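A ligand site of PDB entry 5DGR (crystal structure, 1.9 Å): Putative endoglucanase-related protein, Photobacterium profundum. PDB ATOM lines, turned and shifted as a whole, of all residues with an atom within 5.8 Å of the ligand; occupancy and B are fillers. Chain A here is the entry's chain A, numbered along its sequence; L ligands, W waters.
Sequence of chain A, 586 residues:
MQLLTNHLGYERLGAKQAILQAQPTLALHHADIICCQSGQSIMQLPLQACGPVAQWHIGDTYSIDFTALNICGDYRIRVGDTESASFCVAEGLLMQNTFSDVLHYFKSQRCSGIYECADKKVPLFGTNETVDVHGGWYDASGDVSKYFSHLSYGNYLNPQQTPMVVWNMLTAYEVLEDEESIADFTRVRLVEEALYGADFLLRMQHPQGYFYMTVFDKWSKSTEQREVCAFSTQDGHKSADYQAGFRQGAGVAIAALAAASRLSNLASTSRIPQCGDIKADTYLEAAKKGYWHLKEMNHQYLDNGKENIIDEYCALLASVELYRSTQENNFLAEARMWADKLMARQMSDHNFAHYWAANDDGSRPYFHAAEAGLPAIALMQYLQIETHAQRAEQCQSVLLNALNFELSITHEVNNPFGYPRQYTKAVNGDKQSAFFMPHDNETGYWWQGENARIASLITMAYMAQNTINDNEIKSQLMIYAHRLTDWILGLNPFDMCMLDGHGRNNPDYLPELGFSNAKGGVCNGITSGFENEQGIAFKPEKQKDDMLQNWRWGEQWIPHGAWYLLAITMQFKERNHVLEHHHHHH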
ATOM      1  N   ASP A 139       5.338 -31.542   3.213  1.00  0.00           N
ATOM      2  CA  ASP A 139       4.444 -30.549   3.676  1.00  0.00           C
ATOM      3  C   ASP A 139       3.083 -31.069   4.024  1.00  0.00           C
ATOM      4  O   ASP A 139       2.478 -30.515   4.968  1.00  0.00           O
ATOM      5  CB  ASP A 139       4.319 -29.454   2.569  1.00  0.00           C
ATOM      6  CG  ASP A 139       3.806 -28.109   3.131  1.00  0.00           C
ATOM      7  OD1 ASP A 139       4.405 -27.571   4.068  1.00  0.00           O
ATOM      8  OD2 ASP A 139       2.782 -27.608   2.580  1.00  0.00           O
ATOM      9  N   ALA A 140       2.586 -32.125   3.330  1.00  0.00           N
ATOM     10  CA  ALA A 140       1.173 -32.428   3.464  1.00  0.00           C
ATOM     11  C   ALA A 140       0.957 -33.870   3.130  1.00  0.00           C
ATOM     12  O   ALA A 140       1.859 -34.445   2.477  1.00  0.00           O
ATOM     13  CB  ALA A 140       0.331 -31.517   2.527  1.00  0.00           C
ATOM     14  N   GLY A 142      -0.838 -34.956   0.900  1.00  0.00           N
ATOM     15  CA  GLY A 142      -0.807 -35.058  -0.523  1.00  0.00           C
ATOM     16  C   GLY A 142       0.315 -34.286  -1.213  1.00  0.00           C
ATOM     17  O   GLY A 142       0.187 -33.962  -2.371  1.00  0.00           O
ATOM     18  N   ASP A 143       1.418 -33.978  -0.506  1.00  0.00           N
ATOM     19  CA  ASP A 143       2.442 -33.106  -1.089  1.00  0.00           C
ATOM     20  C   ASP A 143       3.831 -33.407  -0.494  1.00  0.00           C
ATOM     21  O   ASP A 143       4.068 -33.204   0.698  1.00  0.00           O
ATOM     22  CB  ASP A 143       2.029 -31.633  -0.967  1.00  0.00           C
ATOM     23  CG  ASP A 143       2.965 -30.680  -1.727  1.00  0.00           C
ATOM     24  OD1 ASP A 143       3.825 -31.157  -2.511  1.00  0.00           O
ATOM     25  OD2 ASP A 143       2.821 -29.450  -1.568  1.00  0.00           O
ATOM     26  N   TYR A 147       8.544 -26.562   2.334  1.00  0.00           N
ATOM     27  CA  TYR A 147       8.289 -25.124   2.217  1.00  0.00           C
ATOM     28  C   TYR A 147       8.763 -24.390   3.391  1.00  0.00           C
ATOM     29  O   TYR A 147       8.480 -24.781   4.551  1.00  0.00           O
ATOM     30  CB  TYR A 147       6.726 -24.874   2.200  1.00  0.00           C
ATOM     31  CG  TYR A 147       5.947 -25.456   1.097  1.00  0.00           C
ATOM     32  CD1 TYR A 147       5.412 -24.616   0.108  1.00  0.00           C
ATOM     33  CD2 TYR A 147       5.720 -26.879   0.970  1.00  0.00           C
ATOM     34  CE1 TYR A 147       4.637 -25.150  -0.933  1.00  0.00           C
ATOM     35  CE2 TYR A 147       4.910 -27.406  -0.009  1.00  0.00           C
ATOM     36  CZ  TYR A 147       4.429 -26.537  -1.014  1.00  0.00           C
ATOM     37  OH  TYR A 147       3.676 -27.114  -2.038  1.00  0.00           O
ATOM     38  N   HIS A 150       4.543 -20.247   1.140  1.00  0.00           N
ATOM     39  CA  HIS A 150       4.098 -20.050  -0.243  1.00  0.00           C
ATOM     40  C   HIS A 150       2.961 -18.983  -0.230  1.00  0.00           C
ATOM     41  O   HIS A 150       2.783 -18.263   0.772  1.00  0.00           O
ATOM     42  CB  HIS A 150       3.679 -21.394  -0.906  1.00  0.00           C
ATOM     43  CG  HIS A 150       2.394 -21.961  -0.372  1.00  0.00           C
ATOM     44  ND1 HIS A 150       2.207 -22.296   0.970  1.00  0.00           N
ATOM     45  CD2 HIS A 150       1.271 -22.372  -1.021  1.00  0.00           C
ATOM     46  CE1 HIS A 150       0.997 -22.835   1.110  1.00  0.00           C
ATOM     47  NE2 HIS A 150       0.405 -22.876  -0.076  1.00  0.00           N
ATOM     48  N   LEU A 151       2.269 -18.759  -1.360  1.00  0.00           N
ATOM     49  CA  LEU A 151       1.243 -17.670  -1.448  1.00  0.00           C
ATOM     50  C   LEU A 151       1.835 -16.298  -1.355  1.00  0.00           C
ATOM     51  O   LEU A 151       1.117 -15.324  -1.133  1.00  0.00           O
ATOM     52  CB  LEU A 151       0.084 -17.837  -0.364  1.00  0.00           C
ATOM     53  CG  LEU A 151      -0.414 -19.304  -0.224  1.00  0.00           C
ATOM     54  CD1 LEU A 151      -1.423 -19.270   0.949  1.00  0.00           C
ATOM     55  CD2 LEU A 151      -1.073 -19.764  -1.546  1.00  0.00           C
ATOM     56  N   PHE A 216       9.891 -27.477  -4.672  1.00  0.00           N
ATOM     57  CA  PHE A 216       8.539 -27.672  -5.120  1.00  0.00           C
ATOM     58  C   PHE A 216       8.493 -28.530  -6.328  1.00  0.00           C
ATOM     59  O   PHE A 216       9.273 -28.315  -7.351  1.00  0.00           O
ATOM     60  CB  PHE A 216       7.948 -26.320  -5.434  1.00  0.00           C
ATOM     61  CG  PHE A 216       6.540 -26.332  -5.902  1.00  0.00           C
ATOM     62  CD1 PHE A 216       5.534 -26.876  -5.103  1.00  0.00           C
ATOM     63  CD2 PHE A 216       6.165 -25.739  -7.150  1.00  0.00           C
ATOM     64  CE1 PHE A 216       4.198 -26.855  -5.490  1.00  0.00           C
ATOM     65  CE2 PHE A 216       4.825 -25.721  -7.560  1.00  0.00           C
ATOM     66  CZ  PHE A 216       3.823 -26.261  -6.737  1.00  0.00           C
ATOM     67  N   TRP A 219       3.235 -30.502  -7.228  1.00  0.00           N
ATOM     68  CA  TRP A 219       2.310 -31.527  -6.725  1.00  0.00           C
ATOM     69  C   TRP A 219       2.398 -32.829  -7.502  1.00  0.00           C
ATOM     70  O   TRP A 219       1.555 -33.696  -7.366  1.00  0.00           O
ATOM     71  CB  TRP A 219       0.875 -30.990  -6.578  1.00  0.00           C
ATOM     72  CG  TRP A 219       0.820 -29.651  -5.815  1.00  0.00           C
ATOM     73  CD1 TRP A 219       0.890 -29.462  -4.436  1.00  0.00           C
ATOM     74  CD2 TRP A 219       0.576 -28.360  -6.372  1.00  0.00           C
ATOM     75  NE1 TRP A 219       0.735 -28.135  -4.131  1.00  0.00           N
ATOM     76  CE2 TRP A 219       0.546 -27.434  -5.304  1.00  0.00           C
ATOM     77  CE3 TRP A 219       0.355 -27.888  -7.715  1.00  0.00           C
ATOM     78  CZ2 TRP A 219       0.343 -26.068  -5.503  1.00  0.00           C
ATOM     79  CZ3 TRP A 219       0.207 -26.537  -7.923  1.00  0.00           C
ATOM     80  CH2 TRP A 219       0.166 -25.622  -6.839  1.00  0.00           C
ATOM     81  N   PHE A 231       6.351 -20.074  -6.392  1.00  0.00           N
ATOM     82  CA  PHE A 231       5.333 -20.347  -7.399  1.00  0.00           C
ATOM     83  C   PHE A 231       4.083 -19.576  -7.078  1.00  0.00           C
ATOM     84  O   PHE A 231       3.890 -19.151  -5.945  1.00  0.00           O
ATOM     85  CB  PHE A 231       4.986 -21.831  -7.522  1.00  0.00           C
ATOM     86  CG  PHE A 231       4.419 -22.443  -6.237  1.00  0.00           C
ATOM     87  CD1 PHE A 231       3.016 -22.540  -6.036  1.00  0.00           C
ATOM     88  CD2 PHE A 231       5.284 -23.023  -5.281  1.00  0.00           C
ATOM     89  CE1 PHE A 231       2.490 -23.130  -4.852  1.00  0.00           C
ATOM     90  CE2 PHE A 231       4.738 -23.641  -4.131  1.00  0.00           C
ATOM     91  CZ  PHE A 231       3.374 -23.665  -3.926  1.00  0.00           C
ATOM     92  N   TYR A 445      -7.662 -18.107  -5.207  1.00  0.00           N
ATOM     93  CA  TYR A 445      -8.148 -19.507  -5.142  1.00  0.00           C
ATOM     94  C   TYR A 445      -8.083 -20.118  -3.730  1.00  0.00           C
ATOM     95  O   TYR A 445      -8.819 -21.033  -3.483  1.00  0.00           O
ATOM     96  CB  TYR A 445      -7.414 -20.523  -6.069  1.00  0.00           C
ATOM     97  CG  TYR A 445      -6.069 -20.990  -5.531  1.00  0.00           C
ATOM     98  CD1 TYR A 445      -5.925 -22.253  -4.874  1.00  0.00           C
ATOM     99  CD2 TYR A 445      -4.952 -20.171  -5.645  1.00  0.00           C
ATOM    100  CE1 TYR A 445      -4.674 -22.692  -4.334  1.00  0.00           C
ATOM    101  CE2 TYR A 445      -3.737 -20.583  -5.129  1.00  0.00           C
ATOM    102  CZ  TYR A 445      -3.605 -21.851  -4.478  1.00  0.00           C
ATOM    103  OH  TYR A 445      -2.346 -22.181  -4.045  1.00  0.00           O
ATOM    104  N   TRP A 446      -7.118 -19.688  -2.910  1.00  0.00           N
ATOM    105  CA  TRP A 446      -6.725 -20.507  -1.730  1.00  0.00           C
ATOM    106  C   TRP A 446      -7.613 -20.197  -0.520  1.00  0.00           C
ATOM    107  O   TRP A 446      -7.777 -19.039  -0.168  1.00  0.00           O
ATOM    108  CB  TRP A 446      -5.306 -20.227  -1.410  1.00  0.00           C
ATOM    109  CG  TRP A 446      -4.658 -21.160  -0.310  1.00  0.00           C
ATOM    110  CD1 TRP A 446      -4.002 -22.331  -0.524  1.00  0.00           C
ATOM    111  CD2 TRP A 446      -4.604 -20.915   1.077  1.00  0.00           C
ATOM    112  NE1 TRP A 446      -3.465 -22.829   0.653  1.00  0.00           N
ATOM    113  CE2 TRP A 446      -3.864 -22.003   1.674  1.00  0.00           C
ATOM    114  CE3 TRP A 446      -5.117 -19.903   1.917  1.00  0.00           C
ATOM    115  CZ2 TRP A 446      -3.668 -22.118   3.038  1.00  0.00           C
ATOM    116  CZ3 TRP A 446      -4.939 -20.040   3.304  1.00  0.00           C
ATOM    117  CH2 TRP A 446      -4.181 -21.097   3.835  1.00  0.00           C
ATOM    118  N   GLN A 448      -8.935 -22.800   3.182  1.00  0.00           N
ATOM    119  CA  GLN A 448      -9.027 -24.153   3.622  1.00  0.00           C
ATOM    120  C   GLN A 448      -9.424 -24.128   5.122  1.00  0.00           C
ATOM    121  O   GLN A 448      -9.484 -23.050   5.726  1.00  0.00           O
ATOM    122  CB  GLN A 448      -7.647 -24.904   3.452  1.00  0.00           C
ATOM    123  CG  GLN A 448      -6.513 -24.200   4.166  1.00  0.00           C
ATOM    124  CD  GLN A 448      -5.184 -24.860   3.904  1.00  0.00           C
ATOM    125  OE1 GLN A 448      -4.963 -25.481   2.842  1.00  0.00           O
ATOM    126  NE2 GLN A 448      -4.283 -24.795   4.904  1.00  0.00           N
ATOM    127  N   ASN A 524      -6.668 -29.996   7.594  1.00  0.00           N
ATOM    128  CA  ASN A 524      -7.006 -28.551   7.461  1.00  0.00           C
ATOM    129  C   ASN A 524      -8.262 -28.267   8.309  1.00  0.00           C
ATOM    130  O   ASN A 524      -8.244 -27.349   9.122  1.00  0.00           O
ATOM    131  CB  ASN A 524      -7.257 -28.178   5.984  1.00  0.00           C
ATOM    132  CG  ASN A 524      -5.985 -28.261   5.129  1.00  0.00           C
ATOM    133  OD1 ASN A 524      -4.861 -27.987   5.589  1.00  0.00           O
ATOM    134  ND2 ASN A 524      -6.188 -28.497   3.851  1.00  0.00           N
ATOM    135  N   TRP A 551      -8.949 -31.002  -1.317  1.00  0.00           N
ATOM    136  CA  TRP A 551      -7.822 -30.788  -0.430  1.00  0.00           C
ATOM    137  C   TRP A 551      -8.104 -29.729   0.677  1.00  0.00           C
ATOM    138  O   TRP A 551      -7.420 -29.711   1.705  1.00  0.00           O
ATOM    139  CB  TRP A 551      -6.647 -30.306  -1.278  1.00  0.00           C
ATOM    140  CG  TRP A 551      -6.927 -28.959  -2.024  1.00  0.00           C
ATOM    141  CD1 TRP A 551      -7.465 -28.829  -3.280  1.00  0.00           C
ATOM    142  CD2 TRP A 551      -6.699 -27.629  -1.551  1.00  0.00           C
ATOM    143  NE1 TRP A 551      -7.608 -27.497  -3.599  1.00  0.00           N
ATOM    144  CE2 TRP A 551      -7.101 -26.734  -2.584  1.00  0.00           C
ATOM    145  CE3 TRP A 551      -6.140 -27.108  -0.402  1.00  0.00           C
ATOM    146  CZ2 TRP A 551      -7.038 -25.314  -2.456  1.00  0.00           C
ATOM    147  CZ3 TRP A 551      -6.045 -25.679  -0.258  1.00  0.00           C
ATOM    148  CH2 TRP A 551      -6.481 -24.797  -1.330  1.00  0.00           C
ATOM    149  N   ARG A 552      -9.110 -28.882   0.499  1.00  0.00           N
ATOM    150  CA  ARG A 552      -9.404 -27.769   1.439  1.00  0.00           C
ATOM    151  C   ARG A 552      -9.852 -28.288   2.810  1.00  0.00           C
ATOM    152  O   ARG A 552      -9.803 -27.573   3.762  1.00  0.00           O
ATOM    153  CB  ARG A 552     -10.532 -26.867   0.866  1.00  0.00           C
ATOM    154  CG  ARG A 552     -10.059 -26.135  -0.439  1.00  0.00           C
ATOM    155  CD  ARG A 552     -11.288 -25.440  -1.001  1.00  0.00           C
ATOM    156  NE  ARG A 552     -11.062 -24.953  -2.400  1.00  0.00           N
ATOM    157  CZ  ARG A 552     -10.398 -23.878  -2.733  1.00  0.00           C
ATOM    158  NH1 ARG A 552      -9.779 -23.102  -1.831  1.00  0.00           N
ATOM    159  NH2 ARG A 552     -10.405 -23.536  -4.076  1.00  0.00           N
ATOM    160  N   GLU A 555      -7.155 -32.863   3.748  1.00  0.00           N
ATOM    161  CA  GLU A 555      -5.724 -33.018   3.623  1.00  0.00           C
ATOM    162  C   GLU A 555      -5.037 -32.622   4.953  1.00  0.00           C
ATOM    163  O   GLU A 555      -5.425 -31.587   5.577  1.00  0.00           O
ATOM    164  CB  GLU A 555      -5.150 -32.201   2.461  1.00  0.00           C
ATOM    165  CG  GLU A 555      -3.686 -32.584   2.121  1.00  0.00           C
ATOM    166  CD  GLU A 555      -3.115 -31.887   0.880  1.00  0.00           C
ATOM    167  OE1 GLU A 555      -3.680 -30.835   0.438  1.00  0.00           O
ATOM    168  OE2 GLU A 555      -2.057 -32.357   0.398  1.00  0.00           O
ATOM    169  N   GLN A 556      -4.019 -33.386   5.400  1.00  0.00           N
ATOM    170  CA  GLN A 556      -3.093 -32.883   6.463  1.00  0.00           C
ATOM    171  C   GLN A 556      -1.973 -32.001   5.993  1.00  0.00           C
ATOM    172  O   GLN A 556      -1.425 -32.178   4.892  1.00  0.00           O
ATOM    173  CB  GLN A 556      -2.506 -34.040   7.325  1.00  0.00           C
ATOM    174  CG  GLN A 556      -3.649 -35.009   7.877  1.00  0.00           C
ATOM    175  CD  GLN A 556      -3.063 -36.233   8.567  1.00  0.00           C
ATOM    176  OE1 GLN A 556      -2.067 -36.788   8.070  1.00  0.00           O
ATOM    177  NE2 GLN A 556      -3.632 -36.643   9.725  1.00  0.00           N
ATOM    178  N   TRP A 557      -1.567 -31.103   6.884  1.00  0.00           N
ATOM    179  CA  TRP A 557      -0.584 -30.073   6.552  1.00  0.00           C
ATOM    180  C   TRP A 557       0.202 -29.834   7.825  1.00  0.00           C
ATOM    181  O   TRP A 557      -0.394 -29.631   8.927  1.00  0.00           O
ATOM    182  CB  TRP A 557      -1.370 -28.789   6.140  1.00  0.00           C
ATOM    183  CG  TRP A 557      -0.553 -27.707   5.536  1.00  0.00           C
ATOM    184  CD1 TRP A 557       0.489 -27.840   4.602  1.00  0.00           C
ATOM    185  CD2 TRP A 557      -0.733 -26.299   5.761  1.00  0.00           C
ATOM    186  NE1 TRP A 557       0.977 -26.553   4.285  1.00  0.00           N
ATOM    187  CE2 TRP A 557       0.241 -25.611   4.982  1.00  0.00           C
ATOM    188  CE3 TRP A 557      -1.587 -25.556   6.595  1.00  0.00           C
ATOM    189  CZ2 TRP A 557       0.380 -24.191   5.013  1.00  0.00           C
ATOM    190  CZ3 TRP A 557      -1.468 -24.134   6.594  1.00  0.00           C
ATOM    191  CH2 TRP A 557      -0.501 -23.477   5.777  1.00  0.00           C
ATOM    192  N   HIS A 560      -0.594 -27.643  11.034  1.00  0.00           N
ATOM    193  CA  HIS A 560      -1.682 -27.824  11.994  1.00  0.00           C
ATOM    194  C   HIS A 560      -1.121 -28.639  13.164  1.00  0.00           C
ATOM    195  O   HIS A 560      -1.417 -28.356  14.348  1.00  0.00           O
ATOM    196  CB  HIS A 560      -2.852 -28.617  11.388  1.00  0.00           C
ATOM    197  CG  HIS A 560      -3.430 -28.019  10.157  1.00  0.00           C
ATOM    198  ND1 HIS A 560      -3.862 -26.724  10.099  1.00  0.00           N
ATOM    199  CD2 HIS A 560      -3.516 -28.520   8.897  1.00  0.00           C
ATOM    200  CE1 HIS A 560      -4.281 -26.461   8.855  1.00  0.00           C
ATOM    201  NE2 HIS A 560      -4.085 -27.548   8.115  1.00  0.00           N
HETATM  202  C1  LIG L   1       0.003 -28.077  -0.017  1.00  0.00           C
HETATM  203  C2  LIG L   1      -0.445 -26.853  -0.841  1.00  0.00           C
HETATM  204  C3  LIG L   1      -0.966 -25.707   0.119  1.00  0.00           C
HETATM  205  C4  LIG L   1      -2.123 -26.306   1.031  1.00  0.00           C
HETATM  206  C5  LIG L   1      -1.618 -27.604   1.731  1.00  0.00           C
HETATM  207  C6  LIG L   1      -2.720 -28.246   2.664  1.00  0.00           C
HETATM  208  N1  LIG L   1       0.637 -26.345  -1.774  1.00  0.00           N
HETATM  209  O1  LIG L   1       0.109 -29.100  -1.003  1.00  0.00           O
HETATM  210  O2  LIG L   1      -1.519 -24.633  -0.658  1.00  0.00           O
HETATM  211  O3  LIG L   1      -2.437 -25.258   1.956  1.00  0.00           O
HETATM  212  O4  LIG L   1      -1.244 -28.580   0.652  1.00  0.00           O
HETATM  213  O5  LIG L   1      -3.846 -28.613   1.874  1.00  0.00           O
HETATM  214  O   HOH W   1      -2.117 -24.623  -3.004  1.00  0.00           O
HETATM  215  O   HOH W   2      -1.536 -30.798  -1.748  1.00  0.00           O
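An oxygen (O5) of the ligand lies within hydrogen-bond range of the side-chain carboxylate (OE1) of Glu 555 (2.7 Å). A ring nitrogen (NE2) of His 150 is in hydrogen-bond range of an oxygen (O2) of the ligand, 2.7 Å away. The side-chain amide oxygen (OE1) of Gln 448 lies within hydrogen-bond range of an oxygen (O3) of the ligand, at 2.7 Å. OD2 of Asp 143 lies within salt-bridge range of N1 of the ligand (3.8 Å). NE1 of Trp 446 is in hydrogen-bond range of O3 of the ligand, 2.9 Å away. O1 of the ligand lies within hydrogen-bond range of NE1 of Trp 219 (3.3 Å). O5 of the ligand sits at hydrogen-bond distance from ND2 of Asn 524 (3.1 Å). OH of Tyr 147 lies within hydrogen-bond range of N1 of the ligand.
O of Glu 555 lies within hydrogen-bond range of N of Asn 524 (2.9 Å). N of Gly 142 is in hydrogen-bond range of OE2 of Glu 555 (2.9 Å). NE2 of Gln 448 sits at hydrogen-bond distance from OD1 of Asn 524 (3.3 Å). OH of Tyr 147 lies within hydrogen-bond range of OD2 of Asp 143. The side-chain amide nitrogen of Asn 524 lies within hydrogen-bond range of the backbone carbonyl oxygen of Trp 551 (2.8 Å). The side-chain amide oxygen (OD1) of Asn 524 sits at hydrogen-bond distance from a ring nitrogen (NE2) of His 560 (2.7 Å). The side-chain carboxylate (OD2) of Asp 139 sits at hydrogen-bond distance from the indole nitrogen (NE1) of Trp 557 (2.7 Å).
Asp 139 touches the ligand (OD2 to C1, 3.8 Å). Ala 140 touches the ligand. Trp 551 touches the ligand (CE3 to O5, 3.6 Å). Trp 557 touches the ligand (CD1 to C5, 3.6 Å). Hydrophobic or aromatic side chains that line the ligand: Ala 140, Tyr 147, His 150, Trp 219, Trp 446, Trp 551 and Trp 557. 12 residues have an atom within 4 Å of the ligand: Asp 139, Ala 140, Asp 143, Tyr 147, His 150, Trp 219, Trp 446, Gln 448, Asn 524, Trp 551, Glu 555 and Trp 557. Along chain A the residues within 4 Å of the ligand span positions 139 to 557.
Water W1 lies within hydrogen-bond range of O2 of the ligand (2.4 Å) and OH of Tyr 445 (2.7 Å). Water W2 lies within hydrogen-bond range of an oxygen (O1) of the ligand (2.5 Å) and the side-chain carboxylate (OE2) of Glu 555 (2.7 Å).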
